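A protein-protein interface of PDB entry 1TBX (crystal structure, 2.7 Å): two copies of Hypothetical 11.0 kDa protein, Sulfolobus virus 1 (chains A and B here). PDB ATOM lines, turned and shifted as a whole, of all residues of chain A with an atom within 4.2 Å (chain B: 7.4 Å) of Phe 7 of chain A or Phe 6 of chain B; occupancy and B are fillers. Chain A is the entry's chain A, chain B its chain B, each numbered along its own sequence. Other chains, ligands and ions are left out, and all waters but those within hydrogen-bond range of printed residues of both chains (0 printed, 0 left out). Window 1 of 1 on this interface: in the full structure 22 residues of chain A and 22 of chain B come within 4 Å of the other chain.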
ATOM      1  N   THR A   4     -11.687  15.349   7.741  1.00  0.00           N
ATOM      2  CA  THR A   4     -12.172  15.480   9.136  1.00  0.00           C
ATOM      3  C   THR A   4     -12.288  16.940   9.580  1.00  0.00           C
ATOM      4  O   THR A   4     -11.266  17.634   9.700  1.00  0.00           O
ATOM      5  CB  THR A   4     -11.312  14.651  10.129  1.00  0.00           C
ATOM      6  OG1 THR A   4     -11.475  13.264   9.812  1.00  0.00           O
ATOM      7  CG2 THR A   4     -11.846  14.738  11.569  1.00  0.00           C
ATOM      8  N   PRO A   5     -13.529  17.398   9.789  1.00  0.00           N
ATOM      9  CA  PRO A   5     -13.815  18.686  10.480  1.00  0.00           C
ATOM     10  C   PRO A   5     -13.472  18.334  11.913  1.00  0.00           C
ATOM     11  O   PRO A   5     -13.723  17.178  12.262  1.00  0.00           O
ATOM     12  CB  PRO A   5     -15.317  18.838  10.309  1.00  0.00           C
ATOM     13  CG  PRO A   5     -15.760  17.692   9.392  1.00  0.00           C
ATOM     14  CD  PRO A   5     -14.746  16.639   9.439  1.00  0.00           C
ATOM     15  N   PHE A   6     -12.938  19.146  12.798  1.00  0.00           N
ATOM     16  CA  PHE A   6     -13.230  20.440  13.263  1.00  0.00           C
ATOM     17  C   PHE A   6     -11.894  20.449  14.050  1.00  0.00           C
ATOM     18  O   PHE A   6     -11.455  21.465  14.612  1.00  0.00           O
ATOM     19  CB  PHE A   6     -14.287  20.275  14.355  1.00  0.00           C
ATOM     20  CG  PHE A   6     -15.709  20.467  13.894  1.00  0.00           C
ATOM     21  CD1 PHE A   6     -16.385  19.466  13.219  1.00  0.00           C
ATOM     22  CD2 PHE A   6     -16.389  21.653  14.170  1.00  0.00           C
ATOM     23  CE1 PHE A   6     -17.706  19.651  12.788  1.00  0.00           C
ATOM     24  CE2 PHE A   6     -17.690  21.831  13.755  1.00  0.00           C
ATOM     25  CZ  PHE A   6     -18.355  20.820  13.062  1.00  0.00           C
ATOM     26  N   PHE A   7     -11.297  19.241  14.126  1.00  0.00           N
ATOM     27  CA  PHE A   7     -10.051  18.935  14.814  1.00  0.00           C
ATOM     28  C   PHE A   7      -8.966  18.585  13.817  1.00  0.00           C
ATOM     29  O   PHE A   7      -9.166  17.825  12.873  1.00  0.00           O
ATOM     30  CB  PHE A   7     -10.219  17.724  15.746  1.00  0.00           C
ATOM     31  CG  PHE A   7     -11.505  17.730  16.532  1.00  0.00           C
ATOM     32  CD1 PHE A   7     -12.604  17.006  16.087  1.00  0.00           C
ATOM     33  CD2 PHE A   7     -11.632  18.486  17.693  1.00  0.00           C
ATOM     34  CE1 PHE A   7     -13.816  17.004  16.810  1.00  0.00           C
ATOM     35  CE2 PHE A   7     -12.852  18.500  18.418  1.00  0.00           C
ATOM     36  CZ  PHE A   7     -13.946  17.752  17.969  1.00  0.00           C
ATOM     37  N   TYR A   8      -7.800  19.150  14.039  1.00  0.00           N
ATOM     38  CA  TYR A   8      -6.621  18.764  13.321  1.00  0.00           C
ATOM     39  C   TYR A   8      -6.099  17.440  13.885  1.00  0.00           C
ATOM     40  O   TYR A   8      -6.556  16.990  14.947  1.00  0.00           O
ATOM     41  CB  TYR A   8      -5.578  19.834  13.539  1.00  0.00           C
ATOM     42  CG  TYR A   8      -5.669  21.018  12.627  1.00  0.00           C
ATOM     43  CD1 TYR A   8      -6.278  22.213  13.043  1.00  0.00           C
ATOM     44  CD2 TYR A   8      -5.115  20.978  11.368  1.00  0.00           C
ATOM     45  CE1 TYR A   8      -6.315  23.321  12.216  1.00  0.00           C
ATOM     46  CE2 TYR A   8      -5.156  22.062  10.544  1.00  0.00           C
ATOM     47  CZ  TYR A   8      -5.750  23.233  10.958  1.00  0.00           C
ATOM     48  OH  TYR A   8      -5.757  24.310  10.083  1.00  0.00           O
ATOM     49  N   PRO A   9      -5.143  16.811  13.195  1.00  0.00           N
ATOM     50  CA  PRO A   9      -4.558  15.549  13.682  1.00  0.00           C
ATOM     51  C   PRO A   9      -3.948  15.603  15.074  1.00  0.00           C
ATOM     52  O   PRO A   9      -4.140  14.681  15.881  1.00  0.00           O
ATOM     53  CB  PRO A   9      -3.506  15.237  12.645  1.00  0.00           C
ATOM     54  CG  PRO A   9      -4.153  15.787  11.394  1.00  0.00           C
ATOM     55  CD  PRO A   9      -4.628  17.187  11.861  1.00  0.00           C
ATOM     56  N   GLU A  10      -3.233  16.676  15.361  1.00  0.00           N
ATOM     57  CA  GLU A  10      -2.622  16.856  16.664  1.00  0.00           C
ATOM     58  C   GLU A  10      -3.668  16.714  17.772  1.00  0.00           C
ATOM     59  O   GLU A  10      -3.415  16.100  18.827  1.00  0.00           O
ATOM     60  CB  GLU A  10      -2.017  18.232  16.636  1.00  0.00           C
ATOM     61  CG  GLU A  10      -2.029  18.751  15.198  1.00  0.00           C
ATOM     62  CD  GLU A  10      -2.577  20.150  15.101  1.00  0.00           C
ATOM     63  OE1 GLU A  10      -2.896  20.692  16.156  1.00  0.00           O
ATOM     64  OE2 GLU A  10      -2.679  20.735  13.998  1.00  0.00           O
ATOM     65  N   ALA A  11      -4.868  17.252  17.517  1.00  0.00           N
ATOM     66  CA  ALA A  11      -5.970  17.132  18.469  1.00  0.00           C
ATOM     67  C   ALA A  11      -6.436  15.682  18.631  1.00  0.00           C
ATOM     68  O   ALA A  11      -6.590  15.197  19.748  1.00  0.00           O
ATOM     69  CB  ALA A  11      -7.127  18.051  18.080  1.00  0.00           C
ATOM     70  N   LEU A  14      -3.619  13.560  20.270  1.00  0.00           N
ATOM     71  CA  LEU A  14      -3.560  13.895  21.684  1.00  0.00           C
ATOM     72  C   LEU A  14      -4.687  13.249  22.533  1.00  0.00           C
ATOM     73  O   LEU A  14      -4.435  12.647  23.588  1.00  0.00           O
ATOM     74  CB  LEU A  14      -3.549  15.426  21.841  1.00  0.00           C
ATOM     75  CG  LEU A  14      -3.017  15.904  23.193  1.00  0.00           C
ATOM     76  CD1 LEU A  14      -1.678  15.239  23.439  1.00  0.00           C
ATOM     77  CD2 LEU A  14      -2.937  17.446  23.279  1.00  0.00           C
ATOM     78  N   PHE A  49       4.837  17.262  16.227  1.00  0.00           N
ATOM     79  CA  PHE A  49       4.401  18.543  16.720  1.00  0.00           C
ATOM     80  C   PHE A  49       4.148  18.500  18.250  1.00  0.00           C
ATOM     81  O   PHE A  49       4.670  19.323  18.989  1.00  0.00           O
ATOM     82  CB  PHE A  49       3.193  19.019  15.896  1.00  0.00           C
ATOM     83  CG  PHE A  49       2.511  20.223  16.458  1.00  0.00           C
ATOM     84  CD1 PHE A  49       2.959  21.498  16.150  1.00  0.00           C
ATOM     85  CD2 PHE A  49       1.407  20.079  17.305  1.00  0.00           C
ATOM     86  CE1 PHE A  49       2.332  22.619  16.679  1.00  0.00           C
ATOM     87  CE2 PHE A  49       0.763  21.226  17.851  1.00  0.00           C
ATOM     88  CZ  PHE A  49       1.224  22.490  17.530  1.00  0.00           C
ATOM     89  N   LEU A  50       3.390  17.518  18.721  1.00  0.00           N
ATOM     90  CA  LEU A  50       3.050  17.450  20.136  1.00  0.00           C
ATOM     91  C   LEU A  50       4.287  17.232  21.012  1.00  0.00           C
ATOM     92  O   LEU A  50       4.333  17.721  22.153  1.00  0.00           O
ATOM     93  CB  LEU A  50       2.032  16.360  20.379  1.00  0.00           C
ATOM     94  CG  LEU A  50       0.788  16.356  19.481  1.00  0.00           C
ATOM     95  CD1 LEU A  50       0.050  14.984  19.548  1.00  0.00           C
ATOM     96  CD2 LEU A  50      -0.139  17.510  19.893  1.00  0.00           C
ATOM     97  N   PHE A  55       3.619  18.625  24.719  1.00  0.00           N
ATOM     98  CA  PHE A  55       2.437  17.911  25.168  1.00  0.00           C
ATOM     99  C   PHE A  55       2.664  16.420  25.363  1.00  0.00           C
ATOM    100  O   PHE A  55       1.970  15.804  26.163  1.00  0.00           O
ATOM    101  CB  PHE A  55       1.355  18.048  24.147  1.00  0.00           C
ATOM    102  CG  PHE A  55       0.884  19.447  23.954  1.00  0.00           C
ATOM    103  CD1 PHE A  55       1.288  20.184  22.851  1.00  0.00           C
ATOM    104  CD2 PHE A  55      -0.002  20.027  24.848  1.00  0.00           C
ATOM    105  CE1 PHE A  55       0.831  21.468  22.633  1.00  0.00           C
ATOM    106  CE2 PHE A  55      -0.451  21.328  24.636  1.00  0.00           C
ATOM    107  CZ  PHE A  55      -0.029  22.036  23.517  1.00  0.00           C
ATOM    108  N   PHE A  76      -4.833  19.088  28.714  1.00  0.00           N
ATOM    109  CA  PHE A  76      -5.497  19.345  27.428  1.00  0.00           C
ATOM    110  C   PHE A  76      -6.202  18.128  26.828  1.00  0.00           C
ATOM    111  O   PHE A  76      -7.357  18.228  26.407  1.00  0.00           O
ATOM    112  CB  PHE A  76      -4.483  19.874  26.429  1.00  0.00           C
ATOM    113  CG  PHE A  76      -5.084  20.606  25.266  1.00  0.00           C
ATOM    114  CD1 PHE A  76      -6.371  21.142  25.337  1.00  0.00           C
ATOM    115  CD2 PHE A  76      -4.333  20.789  24.093  1.00  0.00           C
ATOM    116  CE1 PHE A  76      -6.924  21.825  24.225  1.00  0.00           C
ATOM    117  CE2 PHE A  76      -4.863  21.476  22.987  1.00  0.00           C
ATOM    118  CZ  PHE A  76      -6.162  21.991  23.054  1.00  0.00           C
ATOM    119  N   LEU A  80     -10.003  17.858  25.092  1.00  0.00           N
ATOM    120  CA  LEU A  80     -10.141  17.434  23.698  1.00  0.00           C
ATOM    121  C   LEU A  80     -10.953  16.139  23.562  1.00  0.00           C
ATOM    122  O   LEU A  80     -11.773  16.035  22.656  1.00  0.00           O
ATOM    123  CB  LEU A  80      -8.779  17.247  23.031  1.00  0.00           C
ATOM    124  CG  LEU A  80      -7.881  18.472  22.735  1.00  0.00           C
ATOM    125  CD1 LEU A  80      -6.435  18.065  22.284  1.00  0.00           C
ATOM    126  CD2 LEU A  80      -8.541  19.511  21.759  1.00  0.00           C
ATOM    127  N   ALA A  83     -14.710  16.836  23.735  1.00  0.00           N
ATOM    128  CA  ALA A  83     -15.058  17.384  22.438  1.00  0.00           C
ATOM    129  C   ALA A  83     -15.176  16.334  21.287  1.00  0.00           C
ATOM    130  O   ALA A  83     -16.254  16.211  20.679  1.00  0.00           O
ATOM    131  CB  ALA A  83     -14.102  18.498  22.083  1.00  0.00           C
ATOM    132  N   ILE A  84     -14.108  15.574  21.002  1.00  0.00           N
ATOM    133  CA  ILE A  84     -14.150  14.510  19.969  1.00  0.00           C
ATOM    134  C   ILE A  84     -15.208  13.448  20.256  1.00  0.00           C
ATOM    135  O   ILE A  84     -15.950  13.001  19.361  1.00  0.00           O
ATOM    136  CB  ILE A  84     -12.784  13.836  19.828  1.00  0.00           C
ATOM    137  CG1 ILE A  84     -11.781  14.817  19.211  1.00  0.00           C
ATOM    138  CG2 ILE A  84     -12.894  12.543  18.998  1.00  0.00           C
ATOM    139  CD1 ILE A  84     -10.414  14.689  19.749  1.00  0.00           C
ATOM    140  N   TYR A  87     -18.477  14.878  19.561  1.00  0.00           N
ATOM    141  CA  TYR A  87     -18.537  14.833  18.099  1.00  0.00           C
ATOM    142  C   TYR A  87     -18.970  13.474  17.556  1.00  0.00           C
ATOM    143  O   TYR A  87     -19.964  13.416  16.817  1.00  0.00           O
ATOM    144  CB  TYR A  87     -17.198  15.151  17.459  1.00  0.00           C
ATOM    145  CG  TYR A  87     -17.292  15.285  15.954  1.00  0.00           C
ATOM    146  CD1 TYR A  87     -18.356  15.974  15.373  1.00  0.00           C
ATOM    147  CD2 TYR A  87     -16.327  14.721  15.111  1.00  0.00           C
ATOM    148  CE1 TYR A  87     -18.467  16.108  14.008  1.00  0.00           C
ATOM    149  CE2 TYR A  87     -16.435  14.852  13.735  1.00  0.00           C
ATOM    150  CZ  TYR A  87     -17.507  15.546  13.190  1.00  0.00           C
ATOM    151  OH  TYR A  87     -17.623  15.724  11.830  1.00  0.00           O
ATOM    152  N   SER B   3      -3.308  28.439  10.215  1.00  0.00           N
ATOM    153  CA  SER B   3      -2.864  29.280  11.329  1.00  0.00           C
ATOM    154  C   SER B   3      -2.791  28.464  12.640  1.00  0.00           C
ATOM    155  O   SER B   3      -1.746  27.854  12.928  1.00  0.00           O
ATOM    156  CB  SER B   3      -3.705  30.579  11.483  1.00  0.00           C
ATOM    157  OG  SER B   3      -4.997  30.536  10.865  1.00  0.00           O
ATOM    158  N   THR B   4      -3.903  28.417  13.383  1.00  0.00           N
ATOM    159  CA  THR B   4      -3.991  27.858  14.732  1.00  0.00           C
ATOM    160  C   THR B   4      -3.871  26.331  14.715  1.00  0.00           C
ATOM    161  O   THR B   4      -4.431  25.685  13.822  1.00  0.00           O
ATOM    162  CB  THR B   4      -5.325  28.346  15.401  1.00  0.00           C
ATOM    163  OG1 THR B   4      -5.279  29.778  15.543  1.00  0.00           O
ATOM    164  CG2 THR B   4      -5.511  27.811  16.850  1.00  0.00           C
ATOM    165  N   PRO B   5      -3.131  25.758  15.681  1.00  0.00           N
ATOM    166  CA  PRO B   5      -2.958  24.301  15.770  1.00  0.00           C
ATOM    167  C   PRO B   5      -4.200  23.424  16.018  1.00  0.00           C
ATOM    168  O   PRO B   5      -4.448  22.587  15.165  1.00  0.00           O
ATOM    169  CB  PRO B   5      -1.926  24.105  16.890  1.00  0.00           C
ATOM    170  CG  PRO B   5      -1.418  25.451  17.254  1.00  0.00           C
ATOM    171  CD  PRO B   5      -2.358  26.459  16.724  1.00  0.00           C
ATOM    172  N   PHE B   6      -4.940  23.473  17.102  1.00  0.00           N
ATOM    173  CA  PHE B   6      -5.622  22.181  17.282  1.00  0.00           C
ATOM    174  C   PHE B   6      -6.950  22.096  16.591  1.00  0.00           C
ATOM    175  O   PHE B   6      -7.505  21.016  16.310  1.00  0.00           O
ATOM    176  CB  PHE B   6      -5.739  21.831  18.739  1.00  0.00           C
ATOM    177  CG  PHE B   6      -4.451  21.441  19.339  1.00  0.00           C
ATOM    178  CD1 PHE B   6      -3.481  22.417  19.627  1.00  0.00           C
ATOM    179  CD2 PHE B   6      -4.179  20.095  19.592  1.00  0.00           C
ATOM    180  CE1 PHE B   6      -2.265  22.065  20.180  1.00  0.00           C
ATOM    181  CE2 PHE B   6      -2.973  19.714  20.150  1.00  0.00           C
ATOM    182  CZ  PHE B   6      -2.000  20.712  20.445  1.00  0.00           C
ATOM    183  N   PHE B   7      -7.422  23.287  16.291  1.00  0.00           N
ATOM    184  CA  PHE B   7      -8.789  23.530  15.928  1.00  0.00           C
ATOM    185  C   PHE B   7      -8.864  24.181  14.534  1.00  0.00           C
ATOM    186  O   PHE B   7      -8.158  25.175  14.239  1.00  0.00           O
ATOM    187  CB  PHE B   7      -9.347  24.499  16.966  1.00  0.00           C
ATOM    188  CG  PHE B   7      -9.195  24.038  18.387  1.00  0.00           C
ATOM    189  CD1 PHE B   7      -8.333  24.691  19.252  1.00  0.00           C
ATOM    190  CD2 PHE B   7      -9.976  22.994  18.888  1.00  0.00           C
ATOM    191  CE1 PHE B   7      -8.223  24.308  20.613  1.00  0.00           C
ATOM    192  CE2 PHE B   7      -9.864  22.572  20.238  1.00  0.00           C
ATOM    193  CZ  PHE B   7      -8.974  23.235  21.098  1.00  0.00           C
ATOM    194  N   TYR B   8      -9.712  23.607  13.688  1.00  0.00           N
ATOM    195  CA  TYR B   8     -10.091  24.197  12.402  1.00  0.00           C
ATOM    196  C   TYR B   8     -11.036  25.359  12.616  1.00  0.00           C
ATOM    197  O   TYR B   8     -11.849  25.325  13.554  1.00  0.00           O
ATOM    198  CB  TYR B   8     -10.852  23.178  11.587  1.00  0.00           C
ATOM    199  CG  TYR B   8      -9.993  22.175  10.893  1.00  0.00           C
ATOM    200  CD1 TYR B   8      -9.853  20.872  11.398  1.00  0.00           C
ATOM    201  CD2 TYR B   8      -9.318  22.511   9.721  1.00  0.00           C
ATOM    202  CE1 TYR B   8      -9.070  19.931  10.748  1.00  0.00           C
ATOM    203  CE2 TYR B   8      -8.512  21.588   9.080  1.00  0.00           C
ATOM    204  CZ  TYR B   8      -8.390  20.300   9.585  1.00  0.00           C
ATOM    205  OH  TYR B   8      -7.590  19.393   8.898  1.00  0.00           O
ATOM    206  N   GLU B  10     -13.955  26.195  11.569  1.00  0.00           N
ATOM    207  CA  GLU B  10     -15.312  25.731  11.953  1.00  0.00           C
ATOM    208  C   GLU B  10     -15.441  25.571  13.446  1.00  0.00           C
ATOM    209  O   GLU B  10     -16.459  25.938  14.022  1.00  0.00           O
ATOM    210  CB  GLU B  10     -15.661  24.315  11.479  1.00  0.00           C
ATOM    211  CG  GLU B  10     -15.306  23.892  10.093  1.00  0.00           C
ATOM    212  CD  GLU B  10     -13.865  23.578   9.994  1.00  0.00           C
ATOM    213  OE1 GLU B  10     -13.131  24.527   9.627  1.00  0.00           O
ATOM    214  OE2 GLU B  10     -13.491  22.419  10.288  1.00  0.00           O
ATOM    215  N   ALA B  11     -14.457  24.890  14.043  1.00  0.00           N
ATOM    216  CA  ALA B  11     -14.493  24.621  15.468  1.00  0.00           C
ATOM    217  C   ALA B  11     -14.463  25.949  16.236  1.00  0.00           C
ATOM    218  O   ALA B  11     -15.256  26.160  17.166  1.00  0.00           O
ATOM    219  CB  ALA B  11     -13.336  23.712  15.880  1.00  0.00           C
ATOM    220  N   ILE B  12     -13.575  26.853  15.840  1.00  0.00           N
ATOM    221  CA  ILE B  12     -13.495  28.127  16.521  1.00  0.00           C
ATOM    222  C   ILE B  12     -14.808  28.919  16.346  1.00  0.00           C
ATOM    223  O   ILE B  12     -15.374  29.446  17.309  1.00  0.00           O
ATOM    224  CB  ILE B  12     -12.334  28.915  15.999  1.00  0.00           C
ATOM    225  CG1 ILE B  12     -11.065  28.104  16.157  1.00  0.00           C
ATOM    226  CG2 ILE B  12     -12.206  30.249  16.768  1.00  0.00           C
ATOM    227  CD1 ILE B  12      -9.935  28.557  15.214  1.00  0.00           C
ATOM    228  N   PHE B  36      -8.240  34.524  17.513  1.00  0.00           N
ATOM    229  CA  PHE B  36      -7.835  33.578  16.473  1.00  0.00           C
ATOM    230  C   PHE B  36      -7.887  34.250  15.151  1.00  0.00           C
ATOM    231  O   PHE B  36      -8.906  34.218  14.456  1.00  0.00           O
ATOM    232  CB  PHE B  36      -8.718  32.345  16.497  1.00  0.00           C
ATOM    233  CG  PHE B  36      -8.567  31.577  17.747  1.00  0.00           C
ATOM    234  CD1 PHE B  36      -9.363  31.866  18.846  1.00  0.00           C
ATOM    235  CD2 PHE B  36      -7.572  30.624  17.863  1.00  0.00           C
ATOM    236  CE1 PHE B  36      -9.206  31.199  20.019  1.00  0.00           C
ATOM    237  CE2 PHE B  36      -7.406  29.941  19.037  1.00  0.00           C
ATOM    238  CZ  PHE B  36      -8.228  30.225  20.118  1.00  0.00           C
ATOM    239  N   PHE B  76     -22.648  20.554  20.710  1.00  0.00           N
ATOM    240  CA  PHE B  76     -21.304  20.467  20.303  1.00  0.00           C
ATOM    241  C   PHE B  76     -20.492  21.710  20.743  1.00  0.00           C
ATOM    242  O   PHE B  76     -19.368  21.577  21.255  1.00  0.00           O
ATOM    243  CB  PHE B  76     -21.270  20.221  18.815  1.00  0.00           C
ATOM    244  CG  PHE B  76     -19.931  19.801  18.318  1.00  0.00           C
ATOM    245  CD1 PHE B  76     -19.044  19.147  19.166  1.00  0.00           C
ATOM    246  CD2 PHE B  76     -19.556  20.042  16.989  1.00  0.00           C
ATOM    247  CE1 PHE B  76     -17.808  18.758  18.714  1.00  0.00           C
ATOM    248  CE2 PHE B  76     -18.325  19.662  16.535  1.00  0.00           C
ATOM    249  CZ  PHE B  76     -17.446  19.017  17.404  1.00  0.00           C
ATOM    250  N   SER B  79     -18.884  21.633  24.340  1.00  0.00           N
ATOM    251  CA  SER B  79     -17.660  20.845  24.496  1.00  0.00           C
ATOM    252  C   SER B  79     -16.474  21.443  23.761  1.00  0.00           C
ATOM    253  O   SER B  79     -15.335  21.347  24.231  1.00  0.00           O
ATOM    254  CB  SER B  79     -17.888  19.409  24.083  1.00  0.00           C
ATOM    255  OG  SER B  79     -17.934  19.299  22.691  1.00  0.00           O
ATOM    256  N   LEU B  80     -16.741  22.073  22.630  1.00  0.00           N
ATOM    257  CA  LEU B  80     -15.699  22.711  21.895  1.00  0.00           C
ATOM    258  C   LEU B  80     -15.138  23.865  22.655  1.00  0.00           C
ATOM    259  O   LEU B  80     -13.946  23.956  22.808  1.00  0.00           O
ATOM    260  CB  LEU B  80     -16.226  23.188  20.572  1.00  0.00           C
ATOM    261  CG  LEU B  80     -16.242  22.187  19.442  1.00  0.00           C
ATOM    262  CD1 LEU B  80     -16.771  22.914  18.210  1.00  0.00           C
ATOM    263  CD2 LEU B  80     -14.847  21.628  19.164  1.00  0.00           C
ATOM    264  N   ALA B  83     -12.660  22.900  25.336  1.00  0.00           N
ATOM    265  CA  ALA B  83     -11.354  22.602  24.776  1.00  0.00           C
ATOM    266  C   ALA B  83     -10.563  23.863  24.374  1.00  0.00           C
ATOM    267  O   ALA B  83      -9.394  23.960  24.713  1.00  0.00           O
ATOM    268  CB  ALA B  83     -11.510  21.674  23.582  1.00  0.00           C
ATOM    269  N   TYR B  87      -7.313  25.326  26.020  1.00  0.00           N
ATOM    270  CA  TYR B  87      -6.158  25.593  25.182  1.00  0.00           C
ATOM    271  C   TYR B  87      -5.553  26.973  25.475  1.00  0.00           C
ATOM    272  O   TYR B  87      -4.337  27.079  25.711  1.00  0.00           O
ATOM    273  CB  TYR B  87      -6.557  25.484  23.727  1.00  0.00           C
ATOM    274  CG  TYR B  87      -5.415  25.755  22.798  1.00  0.00           C
ATOM    275  CD1 TYR B  87      -4.166  25.145  23.011  1.00  0.00           C
ATOM    276  CD2 TYR B  87      -5.566  26.618  21.698  1.00  0.00           C
ATOM    277  CE1 TYR B  87      -3.086  25.360  22.137  1.00  0.00           C
ATOM    278  CE2 TYR B  87      -4.499  26.837  20.799  1.00  0.00           C
ATOM    279  CZ  TYR B  87      -3.250  26.202  21.026  1.00  0.00           C
ATOM    280  OH  TYR B  87      -2.163  26.420  20.178  1.00  0.00           O
ATOM    281  N   LYS B  91      -1.737  27.905  26.695  1.00  0.00           N
ATOM    282  CA  LYS B  91      -0.937  29.001  26.135  1.00  0.00           C
ATOM    283  C   LYS B  91      -0.824  30.157  27.141  1.00  0.00           C
ATOM    284  O   LYS B  91       0.175  30.295  27.846  1.00  0.00           O
ATOM    285  CB  LYS B  91      -1.588  29.496  24.855  1.00  0.00           C
ATOM    286  CG  LYS B  91      -1.529  28.482  23.744  1.00  0.00           C
ATOM    287  CD  LYS B  91      -2.458  28.870  22.599  1.00  0.00           C
ATOM    288  CE  LYS B  91      -1.792  29.735  21.502  1.00  0.00           C
ATOM    289  NZ  LYS B  91      -2.359  31.144  21.596  1.00  0.00           N
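The side-chain carboxylate (OE1) of Glu 10 of chain A lies close to the backbone carbonyl oxygen (O) of Pro 5 of chain B (2.6 Å). The backbone NH (N) of Tyr 8 of chain A sits at hydrogen-bond distance from the backbone carbonyl oxygen (O) of Phe 6 of chain B. N of Tyr 8 of chain B lies within hydrogen-bond range of O of Phe 6 of chain A (2.9 Å).
O of Leu 50 of chain A is in hydrogen-bond range of N of Phe 55 of chain A (2.8 Å). The backbone carbonyl oxygen (O) of Phe 76 of chain B is in hydrogen-bond range of the side-chain hydroxyl (OG) of Ser 79 of chain B (3.1 Å).
Among the printed residues, pairs that only touch across the chains: Thr 4 of chain A with Tyr 8 of chain B, Pro 5 of chain A with Glu 10 of chain B, Phe 6 of chain A with Phe 7 of chain B, Phe 6 of chain A with Glu 10 of chain B, Phe 6 of chain A with Ala 11 of chain B, Phe 6 of chain A with Phe 76 of chain B, Phe 7 of chain A with Phe 6 of chain B, Phe 7 of chain A with Tyr 8 of chain B, Phe 7 of chain A with Phe 76 of chain B, Phe 7 of chain A with Leu 80 of chain B, Tyr 8 of chain A with Thr 4 of chain B, Tyr 8 of chain A with Pro 5 of chain B, Tyr 8 of chain A with Phe 7 of chain B, Tyr 8 of chain A with Tyr 8 of chain B, Glu 10 of chain A with Phe 6 of chain B, Ala 11 of chain A with Phe 6 of chain B, Leu 14 of chain A with Phe 6 of chain B, Phe 49 of chain A with Pro 5 of chain B, Phe 49 of chain A with Phe 6 of chain B, Leu 50 of chain A with Phe 6 of chain B, Phe 55 of chain A with Phe 6 of chain B, Phe 76 of chain A with Phe 6 of chain B, Phe 76 of chain A with Phe 7 of chain B, Phe 76 of chain A with Ala 83 of chain B, Phe 76 of chain A with Tyr 87 of chain B, Leu 80 of chain A with Phe 7 of chain B, Ala 83 of chain A with Phe 76 of chain B, Ala 83 of chain A with Ser 79 of chain B and Tyr 87 of chain A with Phe 76 of chain B.
Pro 9 of chain A touches none of the printed residues of chain B. Of the printed residues of chain A, Pro 5 of chain B touches Tyr 8, Glu 10 and Phe 49. Printed residues of chain A within 4 Å of Phe 6 of chain B: Phe 7 (3.6 Å), Tyr 8 (3.0 Å), Glu 10 (3.3 Å), Ala 11 (3.5 Å), Leu 14 (3.9 Å), Phe 49 (3.8 Å), Leu 50 (3.6 Å), Phe 55 (3.7 Å) and Phe 76 (3.7 Å). Printed residues of chain A within 4 Å of Ala 11 of chain B: Phe 6 (3.2 Å). Printed residues of chain A within 4 Å of Tyr 87 of chain B: Phe 76 (3.6 Å). The nearest residue of chain B that does not touch Phe 7 of chain A is Phe 7 of chain B (4.9 Å). The nearest printed residue of chain B that does not touch Pro 5 of chain A is Tyr 8 of chain B (4.5 Å).
Printed residues of chain A that touch a printed residue of chain B: Thr 4, Pro 5, Phe 6, Phe 7, Tyr 8, Glu 10, Ala 11, Leu 14, Phe 49, Leu 50, Phe 55, Phe 76, Leu 80, Ala 83 and Tyr 87. Hydrophobic or aromatic side chains of chain B within 4 Å of the printed part of chain A: Pro 5, Phe 6, Phe 7, Tyr 8, Ala 11, Phe 76, Leu 80 and Tyr 87. Among the printed residues, 32 pairs touch across the chains.
Thr 4 of chain A touches Tyr 8 of chain B, and with the chains exchanged Tyr 8 of chain A touches Thr 4 of chain B. Phe 6 of chain A touches Phe 76 of chain B, and with the chains exchanged Phe 76 of chain A touches Phe 6 of chain B. Phe 7 of chain A touches Tyr 8 of chain B, and with the chains exchanged Tyr 8 of chain A touches Phe 7 of chain B. Phe 7 of chain A touches Leu 80 of chain B, and with the chains exchanged Leu 80 of chain A touches Phe 7 of chain B.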
